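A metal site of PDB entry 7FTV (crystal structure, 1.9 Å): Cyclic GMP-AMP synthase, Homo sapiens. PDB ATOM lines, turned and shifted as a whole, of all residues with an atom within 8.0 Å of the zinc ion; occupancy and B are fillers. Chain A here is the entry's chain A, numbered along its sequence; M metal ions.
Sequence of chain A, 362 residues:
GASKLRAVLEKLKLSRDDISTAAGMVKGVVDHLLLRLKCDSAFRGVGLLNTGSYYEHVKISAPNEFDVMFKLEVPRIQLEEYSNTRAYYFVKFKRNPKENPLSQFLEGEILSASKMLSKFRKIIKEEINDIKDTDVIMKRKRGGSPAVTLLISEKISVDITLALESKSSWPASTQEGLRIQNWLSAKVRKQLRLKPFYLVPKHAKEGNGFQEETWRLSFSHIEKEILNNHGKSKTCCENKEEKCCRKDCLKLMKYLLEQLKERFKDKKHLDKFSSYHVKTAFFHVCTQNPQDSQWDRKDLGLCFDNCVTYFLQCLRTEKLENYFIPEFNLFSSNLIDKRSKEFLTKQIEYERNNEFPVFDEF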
ATOM      1  N   LEU A 227     -19.274  17.773 -27.525  1.00  0.00           N
ATOM      2  CA  LEU A 227     -18.285  17.424 -28.535  1.00  0.00           C
ATOM      3  C   LEU A 227     -17.155  18.438 -28.566  1.00  0.00           C
ATOM      4  O   LEU A 227     -16.005  18.068 -28.859  1.00  0.00           O
ATOM      5  CB  LEU A 227     -18.963  17.300 -29.901  1.00  0.00           C
ATOM      6  CG  LEU A 227     -19.733  15.979 -30.124  1.00  0.00           C
ATOM      7  CD1 LEU A 227     -20.474  16.026 -31.449  1.00  0.00           C
ATOM      8  CD2 LEU A 227     -18.842  14.705 -30.019  1.00  0.00           C
ATOM      9  N   ASN A 229     -15.920  19.844 -25.903  1.00  0.00           N
ATOM     10  CA  ASN A 229     -15.204  19.749 -24.606  1.00  0.00           C
ATOM     11  C   ASN A 229     -15.467  18.319 -24.110  1.00  0.00           C
ATOM     12  O   ASN A 229     -16.250  18.039 -23.214  1.00  0.00           O
ATOM     13  CB  ASN A 229     -15.663  20.850 -23.630  1.00  0.00           C
ATOM     14  CG  ASN A 229     -14.634  21.146 -22.523  1.00  0.00           C
ATOM     15  OD1 ASN A 229     -13.645  20.431 -22.338  1.00  0.00           O
ATOM     16  ND2 ASN A 229     -14.896  22.184 -21.771  1.00  0.00           N
ATOM     17  N   HIS A 230     -14.789  17.351 -24.758  1.00  0.00           N
ATOM     18  CA  HIS A 230     -15.217  15.962 -24.765  1.00  0.00           C
ATOM     19  C   HIS A 230     -14.296  15.011 -24.001  1.00  0.00           C
ATOM     20  O   HIS A 230     -14.561  13.801 -23.978  1.00  0.00           O
ATOM     21  CB  HIS A 230     -15.297  15.462 -26.227  1.00  0.00           C
ATOM     22  CG  HIS A 230     -13.982  15.559 -26.943  1.00  0.00           C
ATOM     23  ND1 HIS A 230     -13.766  16.457 -27.971  1.00  0.00           N
ATOM     24  CD2 HIS A 230     -12.796  14.947 -26.723  1.00  0.00           C
ATOM     25  CE1 HIS A 230     -12.498  16.367 -28.359  1.00  0.00           C
ATOM     26  NE2 HIS A 230     -11.892  15.450 -27.635  1.00  0.00           N
ATOM     27  N   GLY A 231     -13.192  15.511 -23.440  1.00  0.00           N
ATOM     28  CA  GLY A 231     -12.226  14.606 -22.843  1.00  0.00           C
ATOM     29  C   GLY A 231     -12.456  14.461 -21.357  1.00  0.00           C
ATOM     30  O   GLY A 231     -13.102  15.299 -20.729  1.00  0.00           O
ATOM     31  N   LYS A 232     -11.933  13.375 -20.785  1.00  0.00           N
ATOM     32  CA  LYS A 232     -11.861  13.328 -19.331  1.00  0.00           C
ATOM     33  C   LYS A 232     -10.819  14.312 -18.822  1.00  0.00           C
ATOM     34  O   LYS A 232     -10.997  14.932 -17.762  1.00  0.00           O
ATOM     35  CB  LYS A 232     -11.534  11.915 -18.854  1.00  0.00           C
ATOM     36  CG  LYS A 232     -11.290  11.872 -17.349  1.00  0.00           C
ATOM     37  CD  LYS A 232     -11.035  10.477 -16.849  1.00  0.00           C
ATOM     38  CE  LYS A 232     -12.337   9.828 -16.473  1.00  0.00           C
ATOM     39  NZ  LYS A 232     -13.005  10.610 -15.405  1.00  0.00           N
ATOM     40  N   SER A 233      -9.718  14.463 -19.561  1.00  0.00           N
ATOM     41  CA  SER A 233      -8.739  15.515 -19.296  1.00  0.00           C
ATOM     42  C   SER A 233      -9.237  16.860 -19.833  1.00  0.00           C
ATOM     43  O   SER A 233      -9.789  16.944 -20.930  1.00  0.00           O
ATOM     44  CB  SER A 233      -7.404  15.172 -19.948  1.00  0.00           C
ATOM     45  OG  SER A 233      -6.482  16.251 -19.786  1.00  0.00           O
ATOM     46  N   THR A 235      -7.482  19.116 -21.011  1.00  0.00           N
ATOM     47  CA  THR A 235      -6.662  19.526 -22.151  1.00  0.00           C
ATOM     48  C   THR A 235      -6.794  18.584 -23.352  1.00  0.00           C
ATOM     49  O   THR A 235      -5.978  18.669 -24.277  1.00  0.00           O
ATOM     50  CB  THR A 235      -5.193  19.634 -21.752  1.00  0.00           C
ATOM     51  OG1 THR A 235      -4.786  18.440 -21.074  1.00  0.00           O
ATOM     52  CG2 THR A 235      -4.943  20.850 -20.829  1.00  0.00           C
ATOM     53  N   CYS A 236      -7.755  17.660 -23.339  1.00  0.00           N
ATOM     54  CA  CYS A 236      -7.908  16.730 -24.455  1.00  0.00           C
ATOM     55  C   CYS A 236      -8.012  17.504 -25.759  1.00  0.00           C
ATOM     56  O   CYS A 236      -8.809  18.436 -25.893  1.00  0.00           O
ATOM     57  CB  CYS A 236      -9.155  15.845 -24.263  1.00  0.00           C
ATOM     58  SG  CYS A 236      -9.225  14.369 -25.368  1.00  0.00           S
ATOM     59  N   CYS A 237      -7.152  17.139 -26.718  1.00  0.00           N
ATOM     60  CA  CYS A 237      -7.094  17.667 -28.074  1.00  0.00           C
ATOM     61  C   CYS A 237      -6.599  19.097 -28.171  1.00  0.00           C
ATOM     62  O   CYS A 237      -6.637  19.685 -29.254  1.00  0.00           O
ATOM     63  CB  CYS A 237      -8.454  17.563 -28.778  1.00  0.00           C
ATOM     64  SG  CYS A 237      -8.803  15.857 -29.238  1.00  0.00           S
ATOM     65  N   GLU A 238      -6.077  19.672 -27.072  1.00  0.00           N
ATOM     66  CA  GLU A 238      -5.589  21.044 -27.142  1.00  0.00           C
ATOM     67  C   GLU A 238      -4.201  21.127 -27.757  1.00  0.00           C
ATOM     68  O   GLU A 238      -3.893  22.116 -28.431  1.00  0.00           O
ATOM     69  CB  GLU A 238      -5.611  21.703 -25.759  1.00  0.00           C
ATOM     70  CG  GLU A 238      -7.023  22.130 -25.352  1.00  0.00           C
ATOM     71  CD  GLU A 238      -7.041  23.204 -24.243  1.00  0.00           C
ATOM     72  OE1 GLU A 238      -5.999  23.418 -23.562  1.00  0.00           O
ATOM     73  OE2 GLU A 238      -8.119  23.842 -24.079  1.00  0.00           O
ATOM     74  N   GLU A 242      -1.836  14.543 -26.376  1.00  0.00           N
ATOM     75  CA  GLU A 242      -3.203  14.367 -25.931  1.00  0.00           C
ATOM     76  C   GLU A 242      -4.175  14.550 -27.094  1.00  0.00           C
ATOM     77  O   GLU A 242      -5.152  15.298 -26.995  1.00  0.00           O
ATOM     78  CB  GLU A 242      -3.563  15.346 -24.821  1.00  0.00           C
ATOM     79  CG  GLU A 242      -2.741  15.274 -23.555  1.00  0.00           C
ATOM     80  CD  GLU A 242      -3.452  15.957 -22.394  1.00  0.00           C
ATOM     81  OE1 GLU A 242      -4.704  15.787 -22.303  1.00  0.00           O
ATOM     82  OE2 GLU A 242      -2.783  16.672 -21.602  1.00  0.00           O
ATOM     83  N   LYS A 243      -3.926  13.870 -28.207  1.00  0.00           N
ATOM     84  CA  LYS A 243      -4.807  13.947 -29.367  1.00  0.00           C
ATOM     85  C   LYS A 243      -5.661  12.680 -29.424  1.00  0.00           C
ATOM     86  O   LYS A 243      -5.119  11.574 -29.515  1.00  0.00           O
ATOM     87  CB  LYS A 243      -3.988  14.155 -30.645  1.00  0.00           C
ATOM     88  CG  LYS A 243      -4.520  15.275 -31.507  1.00  0.00           C
ATOM     89  CD  LYS A 243      -6.052  15.287 -31.427  1.00  0.00           C
ATOM     90  CE  LYS A 243      -6.674  16.045 -32.579  1.00  0.00           C
ATOM     91  NZ  LYS A 243      -6.293  17.459 -32.585  1.00  0.00           N
ATOM     92  N   CYS A 244      -6.985  12.830 -29.339  1.00  0.00           N
ATOM     93  CA  CYS A 244      -7.870  11.671 -29.263  1.00  0.00           C
ATOM     94  C   CYS A 244      -8.689  11.508 -30.540  1.00  0.00           C
ATOM     95  O   CYS A 244      -8.811  12.427 -31.359  1.00  0.00           O
ATOM     96  CB  CYS A 244      -8.787  11.747 -28.022  1.00  0.00           C
ATOM     97  SG  CYS A 244     -10.389  12.557 -28.235  1.00  0.00           S
ATOM     98  N   CYS A 245      -9.274  10.321 -30.712  1.00  0.00           N
ATOM     99  CA  CYS A 245     -10.049  10.053 -31.929  1.00  0.00           C
ATOM    100  C   CYS A 245     -11.561   9.982 -31.696  1.00  0.00           C
ATOM    101  O   CYS A 245     -12.280   9.420 -32.528  1.00  0.00           O
ATOM    102  CB  CYS A 245      -9.567   8.772 -32.598  1.00  0.00           C
ATOM    103  SG  CYS A 245      -9.808   7.218 -31.677  1.00  0.00           S
ATOM    104  N   ARG A 246     -12.080  10.589 -30.622  1.00  0.00           N
ATOM    105  CA  ARG A 246     -13.521  10.513 -30.382  1.00  0.00           C
ATOM    106  C   ARG A 246     -14.315  11.125 -31.541  1.00  0.00           C
ATOM    107  O   ARG A 246     -15.220  10.480 -32.096  1.00  0.00           O
ATOM    108  CB  ARG A 246     -13.882  11.197 -29.060  1.00  0.00           C
ATOM    109  CG  ARG A 246     -13.468  10.437 -27.769  1.00  0.00           C
ATOM    110  CD  ARG A 246     -14.059  11.171 -26.575  1.00  0.00           C
ATOM    111  NE  ARG A 246     -13.743  10.577 -25.274  1.00  0.00           N
ATOM    112  CZ  ARG A 246     -12.659  10.854 -24.567  1.00  0.00           C
ATOM    113  NH1 ARG A 246     -11.739  11.701 -25.031  1.00  0.00           N
ATOM    114  NH2 ARG A 246     -12.500  10.308 -23.379  1.00  0.00           N
ATOM    115  N   LYS A 247     -14.005  12.374 -31.915  1.00  0.00           N
ATOM    116  CA  LYS A 247     -14.783  13.028 -32.969  1.00  0.00           C
ATOM    117  C   LYS A 247     -14.672  12.277 -34.296  1.00  0.00           C
ATOM    118  O   LYS A 247     -15.649  12.194 -35.047  1.00  0.00           O
ATOM    119  CB  LYS A 247     -14.351  14.481 -33.141  1.00  0.00           C
ATOM    120  CG  LYS A 247     -14.843  15.427 -32.041  1.00  0.00           C
ATOM    121  CD  LYS A 247     -14.173  16.782 -32.149  1.00  0.00           C
ATOM    122  CE  LYS A 247     -14.915  17.682 -33.086  1.00  0.00           C
ATOM    123  NZ  LYS A 247     -15.059  19.051 -32.472  1.00  0.00           N
ATOM    124  N   ASP A 292      -9.392   9.095 -21.740  1.00  0.00           N
ATOM    125  CA  ASP A 292      -8.826   9.560 -23.013  1.00  0.00           C
ATOM    126  C   ASP A 292      -7.843   8.550 -23.602  1.00  0.00           C
ATOM    127  O   ASP A 292      -7.675   8.507 -24.821  1.00  0.00           O
ATOM    128  CB  ASP A 292      -8.135  10.916 -22.816  1.00  0.00           C
ATOM    129  CG  ASP A 292      -9.093  12.009 -22.341  1.00  0.00           C
ATOM    130  OD1 ASP A 292     -10.324  11.823 -22.474  1.00  0.00           O
ATOM    131  OD2 ASP A 292      -8.618  13.061 -21.868  1.00  0.00           O
ATOM    132  N   TRP A 295      -9.028   6.332 -26.306  1.00  0.00           N
ATOM    133  CA  TRP A 295      -9.354   6.997 -27.562  1.00  0.00           C
ATOM    134  C   TRP A 295      -8.103   7.540 -28.234  1.00  0.00           C
ATOM    135  O   TRP A 295      -8.141   8.603 -28.869  1.00  0.00           O
ATOM    136  CB  TRP A 295     -10.360   8.106 -27.329  1.00  0.00           C
ATOM    137  CG  TRP A 295     -11.659   7.583 -26.795  1.00  0.00           C
ATOM    138  CD1 TRP A 295     -12.009   7.448 -25.495  1.00  0.00           C
ATOM    139  CD2 TRP A 295     -12.765   7.088 -27.568  1.00  0.00           C
ATOM    140  NE1 TRP A 295     -13.271   6.915 -25.393  1.00  0.00           N
ATOM    141  CE2 TRP A 295     -13.760   6.679 -26.655  1.00  0.00           C
ATOM    142  CE3 TRP A 295     -13.022   6.953 -28.948  1.00  0.00           C
ATOM    143  CZ2 TRP A 295     -14.993   6.154 -27.057  1.00  0.00           C
ATOM    144  CZ3 TRP A 295     -14.252   6.444 -29.347  1.00  0.00           C
ATOM    145  CH2 TRP A 295     -15.219   6.047 -28.405  1.00  0.00           C
HETATM  146 ZN    ZN M   1      -9.959  14.785 -27.579  1.00  0.00          ZN
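The zinc ion is bound by NE2 of His 230, 2.0 Å away. SG of Cys 237 is bound to the zinc ion (2.3 Å). SG of Cys 244 is bound to the zinc ion (2.4 Å). SG of Cys 236 binds the zinc ion, at 2.4 Å.
Of the 18 residues printed, 4 come within 4 Å of the zinc ion. The nearest printed residue that does not touch the zinc ion is Arg 246 (4.4 Å).
The backbone carbonyl oxygen of Leu 227 is in hydrogen-bond range of a ring nitrogen (ND1) of His 230 (2.9 Å). The backbone carbonyl oxygen (O) of Glu 242 sits at hydrogen-bond distance from the backbone NH (N) of Cys 237, 2.7 Å away. N of Arg 246 lies close to SG of Cys 244, 3.5 Å away. The guanidinium group (NH1) of Arg 246 lies close to the side-chain sulfur (SG) of Cys 236. SG of Cys 236 sits close to OD2 of Asp 292, 3.8 Å away.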
